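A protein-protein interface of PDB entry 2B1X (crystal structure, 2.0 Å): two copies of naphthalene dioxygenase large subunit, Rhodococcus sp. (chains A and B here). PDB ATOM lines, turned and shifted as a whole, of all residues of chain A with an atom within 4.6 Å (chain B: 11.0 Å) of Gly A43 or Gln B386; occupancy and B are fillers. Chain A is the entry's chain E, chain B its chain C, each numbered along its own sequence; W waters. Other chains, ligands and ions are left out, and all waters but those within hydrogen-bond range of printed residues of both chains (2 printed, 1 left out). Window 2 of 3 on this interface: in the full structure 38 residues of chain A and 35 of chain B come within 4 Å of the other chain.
The side-chain carboxylate (OD2) of Asp A69 sits at hydrogen-bond distance from the backbone NH (N) of Gln B386 (3.2 Å). The side-chain amide nitrogen (NE2) of Gln B386 sits at hydrogen-bond distance from the backbone carbonyl oxygen (O) of Arg A38 (3.1 Å). The backbone NH of Ala B388 is in hydrogen-bond range of the side-chain carboxylate of Asp A69. OD2 of Asp A69 lies within hydrogen-bond range of N of Phe B387, 2.8 Å away.
Water W2 lies within hydrogen-bond range of the side-chain carboxylate (OD2) of Asp A69 (2.6 Å) and the side-chain amide nitrogen (NE2) of Gln B386 (3.0 Å). Water W1 lies within hydrogen-bond range of the backbone carbonyl oxygen of Val B382 (2.8 Å) and the side-chain carboxylate of Asp A69 (2.9 Å).
Hydrophobic or aromatic side chains of chain A within 4 Å of the printed part of chain B: Leu A159. Along chain A the printed residues that touch a printed residue of chain B span positions 38 to 159. Among the printed residues, 8 pairs touch across the chains.
No position is printed for both chains.
Among the printed residues, pairs that only touch across the chains: Asp A69 with Gly B385 (3.0 Å), Glu A39 with Gln B386 (3.6 Å), Leu A159 with Gln B386 (3.8 Å) and Gly A43 with Gln B386 (3.9 Å).
Of the printed residues of chain B, Arg A38 touches Gln B386. Glu A39 touches just one residue of chain B: Gln B386 (3.6 Å). Gly A43 touches one residue of chain B. No residue of chain B comes within 4 Å of His A44. No residue of chain B comes within 4 Å of Ala A45. Printed residues of chain B within 4 Å of Asp A69: Gly B385 (3.0 Å), Gln B386 (3.2 Å), Phe B387 (2.8 Å) and Ala B388 (3.1 Å). Of chain B, only Gln B386 comes within 4 Å of Leu A159. No residue of chain B comes within 4 Å of Asp A160. Met B383 touches none of the printed residues of chain A. Of the printed residues of chain A, Gly B385 touches Asp A69. Printed residues of chain A within 4 Å of Ala B388: Asp A69. The nearest residue of chain B that does not touch Gly A43 is Phe B387 (7.7 Å). The nearest residue of chain A that does not touch Gln B386 is Phe A42 (4.2 Å). The nearest printed residue of chain A that does not touch Gly B385 is Arg A38 (6.5 Å).
ND1 of His A44 sits at hydrogen-bond distance from O of Glu A39, at 3.1 Å. N of Gly A43 lies within hydrogen-bond range of O of Arg A38, at 2.9 Å. The backbone carbonyl oxygen of Phe B387 lies within hydrogen-bond range of the side-chain hydroxyl of Thr B390 (2.8 Å).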
ATOM      1  N   ARG A  38     -14.282  -8.018  39.421  1.00  0.00           N
ATOM      2  CA  ARG A  38     -14.640  -7.835  38.021  1.00  0.00           C
ATOM      3  C   ARG A  38     -14.174  -9.033  37.176  1.00  0.00           C
ATOM      4  O   ARG A  38     -14.949  -9.605  36.417  1.00  0.00           O
ATOM      5  CB  ARG A  38     -13.983  -6.531  37.513  1.00  0.00           C
ATOM      6  CG  ARG A  38     -14.200  -6.271  35.988  1.00  0.00           C
ATOM      7  CD  ARG A  38     -13.453  -4.982  35.461  1.00  0.00           C
ATOM      8  NE  ARG A  38     -14.043  -3.738  35.962  1.00  0.00           N
ATOM      9  CZ  ARG A  38     -13.498  -2.933  36.863  1.00  0.00           C
ATOM     10  NH1 ARG A  38     -12.323  -3.221  37.396  1.00  0.00           N
ATOM     11  NH2 ARG A  38     -14.111  -1.818  37.224  1.00  0.00           N
ATOM     12  N   GLU A  39     -12.922  -9.435  37.347  1.00  0.00           N
ATOM     13  CA  GLU A  39     -12.385 -10.551  36.605  1.00  0.00           C
ATOM     14  C   GLU A  39     -12.873 -11.894  37.197  1.00  0.00           C
ATOM     15  O   GLU A  39     -13.393 -12.731  36.492  1.00  0.00           O
ATOM     16  CB  GLU A  39     -10.842 -10.499  36.618  1.00  0.00           C
ATOM     17  CG  GLU A  39     -10.219 -11.684  35.889  1.00  0.00           C
ATOM     18  CD  GLU A  39      -8.733 -11.817  36.147  1.00  0.00           C
ATOM     19  OE1 GLU A  39      -7.961 -10.934  35.675  1.00  0.00           O
ATOM     20  OE2 GLU A  39      -8.323 -12.793  36.854  1.00  0.00           O
ATOM     21  N   ILE A  41     -15.260 -12.761  39.437  1.00  0.00           N
ATOM     22  CA  ILE A  41     -16.702 -13.069  39.446  1.00  0.00           C
ATOM     23  C   ILE A  41     -17.315 -12.772  38.093  1.00  0.00           C
ATOM     24  O   ILE A  41     -17.812 -13.645  37.459  1.00  0.00           O
ATOM     25  CB  ILE A  41     -17.458 -12.356  40.581  1.00  0.00           C
ATOM     26  CG1 ILE A  41     -17.392 -13.184  41.875  1.00  0.00           C
ATOM     27  CG2 ILE A  41     -18.951 -12.249  40.280  1.00  0.00           C
ATOM     28  CD1 ILE A  41     -16.105 -13.041  42.624  1.00  0.00           C
ATOM     29  N   PHE A  42     -17.277 -11.521  37.655  1.00  0.00           N
ATOM     30  CA  PHE A  42     -18.040 -11.168  36.463  1.00  0.00           C
ATOM     31  C   PHE A  42     -17.393 -11.625  35.162  1.00  0.00           C
ATOM     32  O   PHE A  42     -18.047 -11.686  34.123  1.00  0.00           O
ATOM     33  CB  PHE A  42     -18.393  -9.682  36.471  1.00  0.00           C
ATOM     34  CG  PHE A  42     -19.328  -9.310  37.614  1.00  0.00           C
ATOM     35  CD1 PHE A  42     -18.825  -8.722  38.792  1.00  0.00           C
ATOM     36  CD2 PHE A  42     -20.675  -9.597  37.512  1.00  0.00           C
ATOM     37  CE1 PHE A  42     -19.676  -8.419  39.846  1.00  0.00           C
ATOM     38  CE2 PHE A  42     -21.556  -9.301  38.540  1.00  0.00           C
ATOM     39  CZ  PHE A  42     -21.071  -8.693  39.711  1.00  0.00           C
ATOM     40  N   GLY A  43     -16.127 -12.027  35.251  1.00  0.00           N
ATOM     41  CA  GLY A  43     -15.498 -12.642  34.108  1.00  0.00           C
ATOM     42  C   GLY A  43     -15.719 -14.137  33.996  1.00  0.00           C
ATOM     43  O   GLY A  43     -15.248 -14.747  33.015  1.00  0.00           O
ATOM     44  N   HIS A  44     -16.394 -14.744  34.970  1.00  0.00           N
ATOM     45  CA  HIS A  44     -16.563 -16.201  34.961  1.00  0.00           C
ATOM     46  C   HIS A  44     -18.000 -16.671  35.191  1.00  0.00           C
ATOM     47  O   HIS A  44     -18.432 -17.661  34.601  1.00  0.00           O
ATOM     48  CB  HIS A  44     -15.644 -16.831  36.024  1.00  0.00           C
ATOM     49  CG  HIS A  44     -14.203 -16.836  35.637  1.00  0.00           C
ATOM     50  ND1 HIS A  44     -13.350 -15.796  35.939  1.00  0.00           N
ATOM     51  CD2 HIS A  44     -13.473 -17.731  34.933  1.00  0.00           C
ATOM     52  CE1 HIS A  44     -12.149 -16.061  35.469  1.00  0.00           C
ATOM     53  NE2 HIS A  44     -12.199 -17.224  34.842  1.00  0.00           N
ATOM     54  N   ALA A  45     -18.736 -15.976  36.051  1.00  0.00           N
ATOM     55  CA  ALA A  45     -20.085 -16.448  36.404  1.00  0.00           C
ATOM     56  C   ALA A  45     -21.080 -16.211  35.274  1.00  0.00           C
ATOM     57  O   ALA A  45     -20.777 -15.495  34.319  1.00  0.00           O
ATOM     58  CB  ALA A  45     -20.561 -15.752  37.705  1.00  0.00           C
ATOM     59  N   ASP A  69     -18.612  -4.222  30.017  1.00  0.00           N
ATOM     60  CA  ASP A  69     -18.787  -4.727  28.640  1.00  0.00           C
ATOM     61  C   ASP A  69     -20.232  -4.674  28.190  1.00  0.00           C
ATOM     62  O   ASP A  69     -21.141  -5.116  28.909  1.00  0.00           O
ATOM     63  CB  ASP A  69     -18.253  -6.139  28.514  1.00  0.00           C
ATOM     64  CG  ASP A  69     -16.766  -6.174  28.453  1.00  0.00           C
ATOM     65  OD1 ASP A  69     -16.163  -5.557  27.516  1.00  0.00           O
ATOM     66  OD2 ASP A  69     -16.098  -6.809  29.307  1.00  0.00           O
ATOM     67  N   LEU A 159     -18.564 -14.704  30.316  1.00  0.00           N
ATOM     68  CA  LEU A 159     -17.380 -14.276  29.612  1.00  0.00           C
ATOM     69  C   LEU A 159     -16.352 -15.400  29.477  1.00  0.00           C
ATOM     70  O   LEU A 159     -15.352 -15.227  28.810  1.00  0.00           O
ATOM     71  CB  LEU A 159     -16.764 -13.082  30.362  1.00  0.00           C
ATOM     72  CG  LEU A 159     -17.096 -11.675  29.861  1.00  0.00           C
ATOM     73  CD1 LEU A 159     -18.187 -11.520  28.811  1.00  0.00           C
ATOM     74  CD2 LEU A 159     -17.102 -10.563  30.966  1.00  0.00           C
ATOM     75  N   ASP A 160     -16.600 -16.522  30.126  1.00  0.00           N
ATOM     76  CA  ASP A 160     -15.687 -17.673  30.159  1.00  0.00           C
ATOM     77  C   ASP A 160     -16.113 -18.777  29.180  1.00  0.00           C
ATOM     78  O   ASP A 160     -17.186 -19.383  29.317  1.00  0.00           O
ATOM     79  CB  ASP A 160     -15.674 -18.192  31.587  1.00  0.00           C
ATOM     80  CG  ASP A 160     -14.725 -19.380  31.807  1.00  0.00           C
ATOM     81  OD1 ASP A 160     -14.016 -19.819  30.900  1.00  0.00           O
ATOM     82  OD2 ASP A 160     -14.648 -19.945  32.899  1.00  0.00           O
ATOM     83  N   GLU B   5       1.238  -8.300  32.182  1.00  0.00           N
ATOM     84  CA  GLU B   5       0.135  -8.275  31.222  1.00  0.00           C
ATOM     85  C   GLU B   5       0.344  -7.148  30.189  1.00  0.00           C
ATOM     86  O   GLU B   5       0.219  -7.369  28.985  1.00  0.00           O
ATOM     87  CB  GLU B   5      -1.214  -8.067  31.950  1.00  0.00           C
ATOM     88  CG  GLU B   5      -1.697  -9.240  32.790  1.00  0.00           C
ATOM     89  CD  GLU B   5      -0.848  -9.476  34.044  1.00  0.00           C
ATOM     90  OE1 GLU B   5      -0.350  -8.491  34.668  1.00  0.00           O
ATOM     91  OE2 GLU B   5      -0.669 -10.669  34.410  1.00  0.00           O
ATOM     92  N   THR B   9       1.301  -7.619  26.178  1.00  0.00           N
ATOM     93  CA  THR B   9       0.387  -7.039  25.214  1.00  0.00           C
ATOM     94  C   THR B   9       1.116  -6.143  24.217  1.00  0.00           C
ATOM     95  O   THR B   9       0.895  -6.243  23.013  1.00  0.00           O
ATOM     96  CB  THR B   9      -0.732  -6.266  25.949  1.00  0.00           C
ATOM     97  OG1 THR B   9      -1.566  -7.200  26.667  1.00  0.00           O
ATOM     98  CG2 THR B   9      -1.686  -5.615  24.956  1.00  0.00           C
ATOM     99  N   PRO B  24      -3.524  -4.481  19.493  1.00  0.00           N
ATOM    100  CA  PRO B  24      -4.372  -4.796  20.645  1.00  0.00           C
ATOM    101  C   PRO B  24      -5.288  -3.643  21.031  1.00  0.00           C
ATOM    102  O   PRO B  24      -4.832  -2.499  21.144  1.00  0.00           O
ATOM    103  CB  PRO B  24      -3.369  -5.045  21.786  1.00  0.00           C
ATOM    104  CG  PRO B  24      -2.113  -5.311  21.147  1.00  0.00           C
ATOM    105  CD  PRO B  24      -2.095  -4.639  19.812  1.00  0.00           C
ATOM    106  N   ALA B  25      -6.561  -3.962  21.278  1.00  0.00           N
ATOM    107  CA  ALA B  25      -7.562  -2.973  21.656  1.00  0.00           C
ATOM    108  C   ALA B  25      -7.361  -2.350  23.056  1.00  0.00           C
ATOM    109  O   ALA B  25      -7.899  -1.242  23.362  1.00  0.00           O
ATOM    110  CB  ALA B  25      -8.979  -3.613  21.538  1.00  0.00           C
ATOM    111  N   ALA B  26      -6.585  -3.040  23.898  1.00  0.00           N
ATOM    112  CA  ALA B  26      -6.366  -2.627  25.283  1.00  0.00           C
ATOM    113  C   ALA B  26      -5.637  -1.290  25.376  1.00  0.00           C
ATOM    114  O   ALA B  26      -5.579  -0.696  26.433  1.00  0.00           O
ATOM    115  CB  ALA B  26      -5.568  -3.709  26.074  1.00  0.00           C
ATOM    116  N   ILE B  27      -5.077  -0.806  24.270  1.00  0.00           N
ATOM    117  CA  ILE B  27      -4.367   0.474  24.317  1.00  0.00           C
ATOM    118  C   ILE B  27      -5.246   1.722  24.402  1.00  0.00           C
ATOM    119  O   ILE B  27      -4.737   2.803  24.657  1.00  0.00           O
ATOM    120  CB  ILE B  27      -3.391   0.590  23.129  1.00  0.00           C
ATOM    121  CG1 ILE B  27      -4.136   0.759  21.806  1.00  0.00           C
ATOM    122  CG2 ILE B  27      -2.462  -0.645  23.081  1.00  0.00           C
ATOM    123  CD1 ILE B  27      -3.283   1.341  20.696  1.00  0.00           C
ATOM    124  N   ASN B  29      -8.342   2.644  26.244  1.00  0.00           N
ATOM    125  CA  ASN B  29      -8.907   3.190  27.456  1.00  0.00           C
ATOM    126  C   ASN B  29      -8.539   2.284  28.624  1.00  0.00           C
ATOM    127  O   ASN B  29      -9.253   1.344  28.939  1.00  0.00           O
ATOM    128  CB  ASN B  29     -10.428   3.257  27.317  1.00  0.00           C
ATOM    129  CG  ASN B  29     -11.094   3.810  28.533  1.00  0.00           C
ATOM    130  OD1 ASN B  29     -10.425   4.246  29.483  1.00  0.00           O
ATOM    131  ND2 ASN B  29     -12.431   3.811  28.529  1.00  0.00           N
ATOM    132  N   ASP B  30      -7.423   2.581  29.269  1.00  0.00           N
ATOM    133  CA  ASP B  30      -6.921   1.725  30.342  1.00  0.00           C
ATOM    134  C   ASP B  30      -6.065   2.561  31.286  1.00  0.00           C
ATOM    135  O   ASP B  30      -5.160   3.263  30.828  1.00  0.00           O
ATOM    136  CB  ASP B  30      -6.095   0.564  29.772  1.00  0.00           C
ATOM    137  CG  ASP B  30      -5.660  -0.410  30.849  1.00  0.00           C
ATOM    138  OD1 ASP B  30      -4.478  -0.319  31.321  1.00  0.00           O
ATOM    139  OD2 ASP B  30      -6.447  -1.300  31.290  1.00  0.00           O
ATOM    140  N   PRO B  31      -6.377   2.533  32.581  1.00  0.00           N
ATOM    141  CA  PRO B  31      -5.654   3.364  33.566  1.00  0.00           C
ATOM    142  C   PRO B  31      -4.145   3.075  33.619  1.00  0.00           C
ATOM    143  O   PRO B  31      -3.385   4.034  33.689  1.00  0.00           O
ATOM    144  CB  PRO B  31      -6.332   3.047  34.915  1.00  0.00           C
ATOM    145  CG  PRO B  31      -7.501   2.173  34.610  1.00  0.00           C
ATOM    146  CD  PRO B  31      -7.483   1.743  33.173  1.00  0.00           C
ATOM    147  N   ILE B 379     -16.401   4.843  20.998  1.00  0.00           N
ATOM    148  CA  ILE B 379     -15.318   3.862  21.000  1.00  0.00           C
ATOM    149  C   ILE B 379     -14.737   3.723  22.410  1.00  0.00           C
ATOM    150  O   ILE B 379     -14.607   2.642  22.981  1.00  0.00           O
ATOM    151  CB  ILE B 379     -14.187   4.302  20.030  1.00  0.00           C
ATOM    152  CG1 ILE B 379     -14.697   4.307  18.573  1.00  0.00           C
ATOM    153  CG2 ILE B 379     -12.997   3.397  20.243  1.00  0.00           C
ATOM    154  CD1 ILE B 379     -13.753   4.975  17.534  1.00  0.00           C
ATOM    155  N   THR B 380     -14.413   4.863  22.989  1.00  0.00           N
ATOM    156  CA  THR B 380     -13.722   4.911  24.274  1.00  0.00           C
ATOM    157  C   THR B 380     -14.538   4.210  25.357  1.00  0.00           C
ATOM    158  O   THR B 380     -14.003   3.468  26.213  1.00  0.00           O
ATOM    159  CB  THR B 380     -13.470   6.397  24.622  1.00  0.00           C
ATOM    160  OG1 THR B 380     -12.515   6.928  23.671  1.00  0.00           O
ATOM    161  CG2 THR B 380     -12.793   6.550  26.032  1.00  0.00           C
ATOM    162  N   ARG B 381     -15.841   4.420  25.302  1.00  0.00           N
ATOM    163  CA  ARG B 381     -16.725   3.896  26.318  1.00  0.00           C
ATOM    164  C   ARG B 381     -16.780   2.377  26.254  1.00  0.00           C
ATOM    165  O   ARG B 381     -16.611   1.684  27.268  1.00  0.00           O
ATOM    166  CB  ARG B 381     -18.120   4.475  26.202  1.00  0.00           C
ATOM    167  CG  ARG B 381     -19.074   3.876  27.288  1.00  0.00           C
ATOM    168  CD  ARG B 381     -20.501   4.411  27.249  1.00  0.00           C
ATOM    169  NE  ARG B 381     -21.301   3.822  28.326  1.00  0.00           N
ATOM    170  CZ  ARG B 381     -22.596   3.545  28.249  1.00  0.00           C
ATOM    171  NH1 ARG B 381     -23.291   3.783  27.116  1.00  0.00           N
ATOM    172  NH2 ARG B 381     -23.195   3.035  29.319  1.00  0.00           N
ATOM    173  N   VAL B 382     -16.990   1.852  25.068  1.00  0.00           N
ATOM    174  CA  VAL B 382     -17.094   0.427  24.965  1.00  0.00           C
ATOM    175  C   VAL B 382     -15.722  -0.251  25.128  1.00  0.00           C
ATOM    176  O   VAL B 382     -15.639  -1.375  25.644  1.00  0.00           O
ATOM    177  CB  VAL B 382     -17.980   0.056  23.740  1.00  0.00           C
ATOM    178  CG1 VAL B 382     -17.221   0.126  22.423  1.00  0.00           C
ATOM    179  CG2 VAL B 382     -18.720  -1.234  23.952  1.00  0.00           C
ATOM    180  N   MET B 383     -14.648   0.472  24.799  1.00  0.00           N
ATOM    181  CA  MET B 383     -13.308  -0.067  24.920  1.00  0.00           C
ATOM    182  C   MET B 383     -12.739  -0.086  26.344  1.00  0.00           C
ATOM    183  O   MET B 383     -11.607  -0.536  26.525  1.00  0.00           O
ATOM    184  CB  MET B 383     -12.325   0.665  23.983  1.00  0.00           C
ATOM    185  CG  MET B 383     -12.437   0.237  22.513  1.00  0.00           C
ATOM    186  SD  MET B 383     -12.469  -1.531  22.093  1.00  0.00           S
ATOM    187  CE  MET B 383     -11.339  -2.149  23.068  1.00  0.00           C
ATOM    188  N   GLY B 384     -13.486   0.452  27.321  1.00  0.00           N
ATOM    189  CA  GLY B 384     -13.224   0.227  28.737  1.00  0.00           C
ATOM    190  C   GLY B 384     -13.636  -1.150  29.271  1.00  0.00           C
ATOM    191  O   GLY B 384     -13.247  -1.482  30.387  1.00  0.00           O
ATOM    192  N   GLY B 385     -14.383  -1.952  28.499  1.00  0.00           N
ATOM    193  CA  GLY B 385     -14.754  -3.313  28.935  1.00  0.00           C
ATOM    194  C   GLY B 385     -13.577  -4.319  28.947  1.00  0.00           C
ATOM    195  O   GLY B 385     -12.817  -4.364  28.006  1.00  0.00           O
ATOM    196  N   GLN B 386     -13.478  -5.161  29.976  1.00  0.00           N
ATOM    197  CA  GLN B 386     -12.384  -6.163  30.068  1.00  0.00           C
ATOM    198  C   GLN B 386     -12.347  -7.143  28.909  1.00  0.00           C
ATOM    199  O   GLN B 386     -11.265  -7.523  28.432  1.00  0.00           O
ATOM    200  CB  GLN B 386     -12.405  -6.928  31.387  1.00  0.00           C
ATOM    201  CG  GLN B 386     -13.606  -7.890  31.591  1.00  0.00           C
ATOM    202  CD  GLN B 386     -13.669  -8.420  33.009  1.00  0.00           C
ATOM    203  OE1 GLN B 386     -12.640  -8.507  33.688  1.00  0.00           O
ATOM    204  NE2 GLN B 386     -14.889  -8.754  33.487  1.00  0.00           N
ATOM    205  N   PHE B 387     -13.525  -7.578  28.463  1.00  0.00           N
ATOM    206  CA  PHE B 387     -13.579  -8.450  27.301  1.00  0.00           C
ATOM    207  C   PHE B 387     -13.240  -7.714  25.998  1.00  0.00           C
ATOM    208  O   PHE B 387     -12.484  -8.235  25.131  1.00  0.00           O
ATOM    209  CB  PHE B 387     -14.947  -9.123  27.247  1.00  0.00           C
ATOM    210  CG  PHE B 387     -15.128 -10.037  26.080  1.00  0.00           C
ATOM    211  CD1 PHE B 387     -14.483 -11.258  26.032  1.00  0.00           C
ATOM    212  CD2 PHE B 387     -15.989  -9.674  25.040  1.00  0.00           C
ATOM    213  CE1 PHE B 387     -14.656 -12.150  24.936  1.00  0.00           C
ATOM    214  CE2 PHE B 387     -16.182 -10.558  23.932  1.00  0.00           C
ATOM    215  CZ  PHE B 387     -15.499 -11.811  23.904  1.00  0.00           C
ATOM    216  N   ALA B 388     -13.750  -6.493  25.859  1.00  0.00           N
ATOM    217  CA  ALA B 388     -13.506  -5.716  24.646  1.00  0.00           C
ATOM    218  C   ALA B 388     -12.007  -5.515  24.463  1.00  0.00           C
ATOM    219  O   ALA B 388     -11.491  -5.468  23.351  1.00  0.00           O
ATOM    220  CB  ALA B 388     -14.206  -4.376  24.715  1.00  0.00           C
ATOM    221  N   LYS B 389     -11.313  -5.460  25.573  1.00  0.00           N
ATOM    222  CA  LYS B 389      -9.870  -5.148  25.593  1.00  0.00           C
ATOM    223  C   LYS B 389      -8.963  -6.321  25.231  1.00  0.00           C
ATOM    224  O   LYS B 389      -7.752  -6.119  24.996  1.00  0.00           O
ATOM    225  CB  LYS B 389      -9.485  -4.715  26.993  1.00  0.00           C
ATOM    226  CG  LYS B 389      -9.694  -3.240  27.314  1.00  0.00           C
ATOM    227  CD  LYS B 389      -9.307  -3.113  28.795  1.00  0.00           C
ATOM    228  CE  LYS B 389      -9.183  -1.680  29.231  1.00  0.00           C
ATOM    229  NZ  LYS B 389      -9.193  -1.611  30.695  1.00  0.00           N
ATOM    230  N   THR B 390      -9.515  -7.528  25.227  1.00  0.00           N
ATOM    231  CA  THR B 390      -8.784  -8.704  24.758  1.00  0.00           C
ATOM    232  C   THR B 390      -8.819  -8.838  23.246  1.00  0.00           C
ATOM    233  O   THR B 390      -8.237  -9.750  22.713  1.00  0.00           O
ATOM    234  CB  THR B 390      -9.320  -9.985  25.412  1.00  0.00           C
ATOM    235  OG1 THR B 390     -10.640 -10.283  24.923  1.00  0.00           O
ATOM    236  CG2 THR B 390      -9.490  -9.784  26.941  1.00  0.00           C
ATOM    237  N   GLY B 391      -9.551  -7.957  22.566  1.00  0.00           N
ATOM    238  CA  GLY B 391      -9.625  -8.001  21.123  1.00  0.00           C
ATOM    239  C   GLY B 391      -8.565  -7.154  20.434  1.00  0.00           C
ATOM    240  O   GLY B 391      -7.649  -6.610  21.058  1.00  0.00           O
ATOM    241  N   GLU B 392      -8.716  -7.029  19.126  1.00  0.00           N
ATOM    242  CA  GLU B 392      -7.737  -6.318  18.326  1.00  0.00           C
ATOM    243  C   GLU B 392      -8.443  -5.247  17.518  1.00  0.00           C
ATOM    244  O   GLU B 392      -9.662  -5.299  17.305  1.00  0.00           O
ATOM    245  CB  GLU B 392      -6.975  -7.312  17.421  1.00  0.00           C
ATOM    246  CG  GLU B 392      -7.836  -7.952  16.343  1.00  0.00           C
ATOM    247  CD  GLU B 392      -8.638  -9.171  16.814  1.00  0.00           C
ATOM    248  OE1 GLU B 392      -9.726  -9.000  17.409  1.00  0.00           O
ATOM    249  OE2 GLU B 392      -8.201 -10.318  16.559  1.00  0.00           O
HETATM  250  O   HOH W   1     -17.458  -3.417  25.979  1.00  0.00           O
HETATM  251  O   HOH W   2     -16.811  -7.154  31.810  1.00  0.00           O
